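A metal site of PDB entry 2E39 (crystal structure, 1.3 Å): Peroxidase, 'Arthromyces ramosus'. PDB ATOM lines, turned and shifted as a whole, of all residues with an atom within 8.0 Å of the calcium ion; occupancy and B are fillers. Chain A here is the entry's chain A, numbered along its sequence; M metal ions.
Five residues have an atom within 4 Å of the calcium ion: Ser 185, Asp 202, Thr 204, Val 207 and Asp 209. The nearest printed residue that does not touch the calcium ion is Pro 205 (4.3 Å).
N of Phe 212 sits close to OD2 of Asp 202, at 2.9 Å. The backbone NH (N) of Gln 211 sits close to the side-chain carboxylate (OD1) of Asp 209, at 3.4 Å.
The calcium ion is bound by the backbone carbonyl oxygen (O) of Thr 204 (2.4 Å). The backbone carbonyl oxygen (O) of Ser 185 is bound to the calcium ion, 2.4 Å away. O of Val 207 is bound to the calcium ion, 2.4 Å away. The calcium ion is bound by the side-chain carboxylate (OD2) of Asp 202 (2.5 Å). OD1 of Asp 209 is bound to the calcium ion (2.5 Å). The calcium ion is bound by OG of Ser 185 (2.5 Å). OG1 of Thr 204 binds the calcium ion. OD1 of Asp 202 is bound to the calcium ion, 2.7 Å away.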
ATOM      1  N   PRO A 130      18.291   8.754   6.261  1.00  0.00           N
ATOM      2  CA  PRO A 130      17.358   9.592   5.522  1.00  0.00           C
ATOM      3  C   PRO A 130      17.971  10.835   4.926  1.00  0.00           C
ATOM      4  O   PRO A 130      18.753  11.513   5.559  1.00  0.00           O
ATOM      5  CB  PRO A 130      16.372   9.963   6.643  1.00  0.00           C
ATOM      6  CG  PRO A 130      16.300   8.711   7.486  1.00  0.00           C
ATOM      7  CD  PRO A 130      17.775   8.311   7.563  1.00  0.00           C
ATOM      8  N   ALA A 182      29.957  17.561   4.676  1.00  0.00           N
ATOM      9  CA  ALA A 182      28.555  17.217   4.849  1.00  0.00           C
ATOM     10  C   ALA A 182      28.424  15.971   5.715  1.00  0.00           C
ATOM     11  O   ALA A 182      27.378  15.807   6.366  1.00  0.00           O
ATOM     12  CB  ALA A 182      27.862  17.059   3.506  1.00  0.00           C
ATOM     13  N   ALA A 183      29.429  15.099   5.730  1.00  0.00           N
ATOM     14  CA  ALA A 183      29.413  13.933   6.605  1.00  0.00           C
ATOM     15  C   ALA A 183      29.218  14.311   8.059  1.00  0.00           C
ATOM     16  O   ALA A 183      28.696  13.501   8.866  1.00  0.00           O
ATOM     17  CB  ALA A 183      30.697  13.138   6.425  1.00  0.00           C
ATOM     18  N   HIS A 184      29.618  15.508   8.492  1.00  0.00           N
ATOM     19  CA  HIS A 184      29.403  15.927   9.878  1.00  0.00           C
ATOM     20  C   HIS A 184      27.940  16.204  10.167  1.00  0.00           C
ATOM     21  O   HIS A 184      27.582  16.465  11.322  1.00  0.00           O
ATOM     22  CB  HIS A 184      30.328  17.091  10.224  1.00  0.00           C
ATOM     23  CG  HIS A 184      31.738  16.672  10.523  1.00  0.00           C
ATOM     24  ND1 HIS A 184      32.663  17.522  11.115  1.00  0.00           N
ATOM     25  CD2 HIS A 184      32.422  15.527  10.301  1.00  0.00           C
ATOM     26  CE1 HIS A 184      33.822  16.863  11.250  1.00  0.00           C
ATOM     27  NE2 HIS A 184      33.705  15.622  10.754  1.00  0.00           N
ATOM     28  N   SER A 185      27.065  16.078   9.160  1.00  0.00           N
ATOM     29  CA  SER A 185      25.629  16.029   9.359  1.00  0.00           C
ATOM     30  C   SER A 185      25.169  14.712   9.981  1.00  0.00           C
ATOM     31  O   SER A 185      24.024  14.603  10.444  1.00  0.00           O
ATOM     32  CB  SER A 185      24.897  16.206   8.033  1.00  0.00           C
ATOM     33  OG  SER A 185      23.529  16.469   8.254  1.00  0.00           O
ATOM     34  N   LEU A 186      26.034  13.706  10.015  1.00  0.00           N
ATOM     35  CA  LEU A 186      25.710  12.397  10.548  1.00  0.00           C
ATOM     36  C   LEU A 186      26.788  12.056  11.589  1.00  0.00           C
ATOM     37  O   LEU A 186      27.560  11.132  11.367  1.00  0.00           O
ATOM     38  CB  LEU A 186      25.697  11.340   9.461  1.00  0.00           C
ATOM     39  CG  LEU A 186      24.649  11.461   8.370  1.00  0.00           C
ATOM     40  CD1 LEU A 186      24.988  10.440   7.252  1.00  0.00           C
ATOM     41  CD2 LEU A 186      23.230  11.284   8.881  1.00  0.00           C
ATOM     42  N   ALA A 187      26.874  12.817  12.688  1.00  0.00           N
ATOM     43  CA  ALA A 187      28.115  12.806  13.424  1.00  0.00           C
ATOM     44  C   ALA A 187      28.002  13.159  14.887  1.00  0.00           C
ATOM     45  O   ALA A 187      27.148  13.940  15.285  1.00  0.00           O
ATOM     46  CB  ALA A 187      29.117  13.796  12.762  1.00  0.00           C
ATOM     47  N   LEU A 201      27.220  16.563  16.416  1.00  0.00           N
ATOM     48  CA  LEU A 201      27.698  17.783  15.781  1.00  0.00           C
ATOM     49  C   LEU A 201      26.584  18.619  15.171  1.00  0.00           C
ATOM     50  O   LEU A 201      26.778  19.818  14.848  1.00  0.00           O
ATOM     51  CB  LEU A 201      28.778  17.482  14.757  1.00  0.00           C
ATOM     52  CG  LEU A 201      29.941  16.582  15.168  1.00  0.00           C
ATOM     53  CD1 LEU A 201      30.991  16.516  14.077  1.00  0.00           C
ATOM     54  CD2 LEU A 201      30.536  17.081  16.485  1.00  0.00           C
ATOM     55  N   ASP A 202      25.417  18.039  14.928  1.00  0.00           N
ATOM     56  CA  ASP A 202      24.218  18.778  14.501  1.00  0.00           C
ATOM     57  C   ASP A 202      23.010  18.151  15.179  1.00  0.00           C
ATOM     58  O   ASP A 202      23.092  17.076  15.780  1.00  0.00           O
ATOM     59  CB  ASP A 202      24.076  18.913  12.987  1.00  0.00           C
ATOM     60  CG  ASP A 202      23.422  17.841  12.144  1.00  0.00           C
ATOM     61  OD1 ASP A 202      22.953  16.805  12.660  1.00  0.00           O
ATOM     62  OD2 ASP A 202      23.354  18.054  10.894  1.00  0.00           O
ATOM     63  N   SER A 203      21.885  18.866  15.109  1.00  0.00           N
ATOM     64  CA  SER A 203      20.705  18.450  15.862  1.00  0.00           C
ATOM     65  C   SER A 203      20.061  17.197  15.238  1.00  0.00           C
ATOM     66  O   SER A 203      19.161  16.628  15.872  1.00  0.00           O
ATOM     67  CB  SER A 203      19.694  19.594  15.918  1.00  0.00           C
ATOM     68  OG  SER A 203      19.230  19.945  14.619  1.00  0.00           O
ATOM     69  N   THR A 204      20.500  16.758  14.070  1.00  0.00           N
ATOM     70  CA  THR A 204      19.912  15.610  13.401  1.00  0.00           C
ATOM     71  C   THR A 204      20.957  14.602  12.954  1.00  0.00           C
ATOM     72  O   THR A 204      21.222  14.375  11.765  1.00  0.00           O
ATOM     73  CB  THR A 204      19.071  16.073  12.183  1.00  0.00           C
ATOM     74  OG1 THR A 204      19.947  16.825  11.314  1.00  0.00           O
ATOM     75  CG2 THR A 204      17.877  16.930  12.583  1.00  0.00           C
ATOM     76  N   PRO A 205      21.614  13.927  13.911  1.00  0.00           N
ATOM     77  CA  PRO A 205      22.722  13.020  13.521  1.00  0.00           C
ATOM     78  C   PRO A 205      22.279  11.748  12.824  1.00  0.00           C
ATOM     79  O   PRO A 205      23.150  11.003  12.356  1.00  0.00           O
ATOM     80  CB  PRO A 205      23.400  12.694  14.861  1.00  0.00           C
ATOM     81  CG  PRO A 205      22.286  12.839  15.886  1.00  0.00           C
ATOM     82  CD  PRO A 205      21.507  14.009  15.370  1.00  0.00           C
ATOM     83  N   GLN A 206      20.979  11.569  12.664  1.00  0.00           N
ATOM     84  CA  GLN A 206      20.479  10.474  11.845  1.00  0.00           C
ATOM     85  C   GLN A 206      19.759  10.946  10.611  1.00  0.00           C
ATOM     86  O   GLN A 206      19.024  10.170   9.973  1.00  0.00           O
ATOM     87  CB  GLN A 206      19.515   9.584  12.633  1.00  0.00           C
ATOM     88  CG  GLN A 206      20.167   8.935  13.853  1.00  0.00           C
ATOM     89  CD  GLN A 206      19.191   7.984  14.514  1.00  0.00           C
ATOM     90  OE1 GLN A 206      18.338   8.403  15.290  1.00  0.00           O
ATOM     91  NE2 GLN A 206      19.353   6.707  14.205  1.00  0.00           N
ATOM     92  N   VAL A 207      19.883  12.214  10.237  1.00  0.00           N
ATOM     93  CA  VAL A 207      19.367  12.738   8.985  1.00  0.00           C
ATOM     94  C   VAL A 207      20.465  13.480   8.225  1.00  0.00           C
ATOM     95  O   VAL A 207      21.126  14.349   8.765  1.00  0.00           O
ATOM     96  CB  VAL A 207      18.136  13.647   9.190  1.00  0.00           C
ATOM     97  CG1 VAL A 207      17.593  14.129   7.832  1.00  0.00           C
ATOM     98  CG2 VAL A 207      17.034  12.962   9.978  1.00  0.00           C
ATOM     99  N   PHE A 208      20.695  13.095   6.972  1.00  0.00           N
ATOM    100  CA  PHE A 208      21.680  13.695   6.093  1.00  0.00           C
ATOM    101  C   PHE A 208      21.079  14.961   5.503  1.00  0.00           C
ATOM    102  O   PHE A 208      20.353  14.885   4.520  1.00  0.00           O
ATOM    103  CB  PHE A 208      22.144  12.740   5.016  1.00  0.00           C
ATOM    104  CG  PHE A 208      23.306  13.352   4.234  1.00  0.00           C
ATOM    105  CD1 PHE A 208      24.572  13.428   4.772  1.00  0.00           C
ATOM    106  CD2 PHE A 208      23.120  13.815   2.948  1.00  0.00           C
ATOM    107  CE1 PHE A 208      25.606  13.950   4.033  1.00  0.00           C
ATOM    108  CE2 PHE A 208      24.138  14.336   2.216  1.00  0.00           C
ATOM    109  CZ  PHE A 208      25.406  14.399   2.757  1.00  0.00           C
ATOM    110  N   ASP A 209      21.317  16.095   6.143  1.00  0.00           N
ATOM    111  CA  ASP A 209      20.641  17.369   5.895  1.00  0.00           C
ATOM    112  C   ASP A 209      21.617  18.511   6.127  1.00  0.00           C
ATOM    113  O   ASP A 209      22.805  18.350   6.499  1.00  0.00           O
ATOM    114  CB  ASP A 209      19.384  17.524   6.748  1.00  0.00           C
ATOM    115  CG  ASP A 209      19.670  17.413   8.240  1.00  0.00           C
ATOM    116  OD1 ASP A 209      20.862  17.478   8.639  1.00  0.00           O
ATOM    117  OD2 ASP A 209      18.694  17.300   9.044  1.00  0.00           O
ATOM    118  N   THR A 210      21.139  19.743   5.890  1.00  0.00           N
ATOM    119  CA  THR A 210      22.012  20.911   6.001  1.00  0.00           C
ATOM    120  C   THR A 210      22.146  21.444   7.439  1.00  0.00           C
ATOM    121  O   THR A 210      22.771  22.468   7.603  1.00  0.00           O
ATOM    122  CB  THR A 210      21.458  22.060   5.147  1.00  0.00           C
ATOM    123  OG1 THR A 210      20.209  22.447   5.683  1.00  0.00           O
ATOM    124  CG2 THR A 210      21.247  21.648   3.694  1.00  0.00           C
ATOM    125  N   GLN A 211      21.593  20.784   8.464  1.00  0.00           N
ATOM    126  CA  GLN A 211      21.608  21.344   9.789  1.00  0.00           C
ATOM    127  C   GLN A 211      23.031  21.639  10.260  1.00  0.00           C
ATOM    128  O   GLN A 211      23.255  22.659  10.913  1.00  0.00           O
ATOM    129  CB  GLN A 211      20.872  20.444  10.805  1.00  0.00           C
ATOM    130  CG  GLN A 211      19.366  20.359  10.668  1.00  0.00           C
ATOM    131  CD  GLN A 211      18.697  21.716  10.613  1.00  0.00           C
ATOM    132  OE1 GLN A 211      17.910  21.946   9.681  1.00  0.00           O
ATOM    133  NE2 GLN A 211      18.988  22.632  11.536  1.00  0.00           N
ATOM    134  N   PHE A 212      23.982  20.748   9.944  1.00  0.00           N
ATOM    135  CA  PHE A 212      25.369  20.964  10.343  1.00  0.00           C
ATOM    136  C   PHE A 212      25.877  22.319   9.922  1.00  0.00           C
ATOM    137  O   PHE A 212      26.559  23.033  10.690  1.00  0.00           O
ATOM    138  CB  PHE A 212      26.256  19.834   9.789  1.00  0.00           C
ATOM    139  CG  PHE A 212      27.736  20.098   9.920  1.00  0.00           C
ATOM    140  CD1 PHE A 212      28.375  20.022  11.160  1.00  0.00           C
ATOM    141  CD2 PHE A 212      28.489  20.434   8.829  1.00  0.00           C
ATOM    142  CE1 PHE A 212      29.719  20.294  11.263  1.00  0.00           C
ATOM    143  CE2 PHE A 212      29.819  20.726   8.928  1.00  0.00           C
ATOM    144  CZ  PHE A 212      30.431  20.657  10.151  1.00  0.00           C
ATOM    145  N   TYR A 213      25.633  22.722   8.687  1.00  0.00           N
ATOM    146  CA  TYR A 213      26.132  23.973   8.173  1.00  0.00           C
ATOM    147  C   TYR A 213      25.468  25.163   8.825  1.00  0.00           C
ATOM    148  O   TYR A 213      26.131  26.169   9.078  1.00  0.00           O
ATOM    149  CB  TYR A 213      25.970  24.015   6.648  1.00  0.00           C
ATOM    150  CG  TYR A 213      26.787  22.985   5.898  1.00  0.00           C
ATOM    151  CD1 TYR A 213      28.133  23.160   5.683  1.00  0.00           C
ATOM    152  CD2 TYR A 213      26.198  21.836   5.408  1.00  0.00           C
ATOM    153  CE1 TYR A 213      28.913  22.235   5.024  1.00  0.00           C
ATOM    154  CE2 TYR A 213      26.966  20.936   4.738  1.00  0.00           C
ATOM    155  CZ  TYR A 213      28.319  21.107   4.536  1.00  0.00           C
ATOM    156  OH  TYR A 213      28.980  20.161   3.806  1.00  0.00           O
ATOM    157  N   GLU A 215      24.019  25.141  11.923  1.00  0.00           N
ATOM    158  CA  GLU A 215      24.215  25.236  13.368  1.00  0.00           C
ATOM    159  C   GLU A 215      25.644  25.593  13.757  1.00  0.00           C
ATOM    160  O   GLU A 215      25.862  26.234  14.787  1.00  0.00           O
ATOM    161  CB  GLU A 215      23.765  23.925  14.035  1.00  0.00           C
ATOM    162  CG  GLU A 215      22.254  23.745  13.904  1.00  0.00           C
ATOM    163  CD  GLU A 215      21.736  22.388  14.255  1.00  0.00           C
ATOM    164  OE1 GLU A 215      22.430  21.588  14.952  1.00  0.00           O
ATOM    165  OE2 GLU A 215      20.616  22.057  13.813  1.00  0.00           O
ATOM    166  N   ASN A 266      19.143  20.828   0.773  1.00  0.00           N
ATOM    167  CA  ASN A 266      19.593  19.452   0.905  1.00  0.00           C
ATOM    168  C   ASN A 266      19.950  18.803  -0.434  1.00  0.00           C
ATOM    169  O   ASN A 266      20.853  17.978  -0.485  1.00  0.00           O
ATOM    170  CB  ASN A 266      18.485  18.654   1.620  1.00  0.00           C
ATOM    171  CG  ASN A 266      18.216  19.010   3.071  1.00  0.00           C
ATOM    172  OD1 ASN A 266      19.137  19.165   3.843  1.00  0.00           O
ATOM    173  ND2 ASN A 266      16.949  19.105   3.436  1.00  0.00           N
ATOM    174  N   MET A 269      23.385  20.070  -1.566  1.00  0.00           N
ATOM    175  CA  MET A 269      24.347  19.479  -0.659  1.00  0.00           C
ATOM    176  C   MET A 269      24.629  18.024  -1.033  1.00  0.00           C
ATOM    177  O   MET A 269      25.792  17.590  -1.116  1.00  0.00           O
ATOM    178  CB  MET A 269      23.868  19.550   0.790  1.00  0.00           C
ATOM    179  CG  MET A 269      24.846  18.945   1.783  1.00  0.00           C
ATOM    180  SD  MET A 269      24.173  18.835   3.444  1.00  0.00           S
ATOM    181  CE  MET A 269      22.978  17.526   3.129  1.00  0.00           C
ATOM    182  N   ASN A 303      14.117  12.445   2.924  1.00  0.00           N
ATOM    183  CA  ASN A 303      13.972  13.315   4.088  1.00  0.00           C
ATOM    184  C   ASN A 303      12.999  14.419   3.688  1.00  0.00           C
ATOM    185  O   ASN A 303      13.299  15.157   2.762  1.00  0.00           O
ATOM    186  CB  ASN A 303      15.298  13.918   4.546  1.00  0.00           C
ATOM    187  CG  ASN A 303      15.149  15.027   5.549  1.00  0.00           C
ATOM    188  OD1 ASN A 303      14.256  14.959   6.416  1.00  0.00           O
ATOM    189  ND2 ASN A 303      15.971  16.086   5.471  1.00  0.00           N
HETATM  190 CA    CA M   1      22.078  16.050  10.242  1.00  0.00          CA
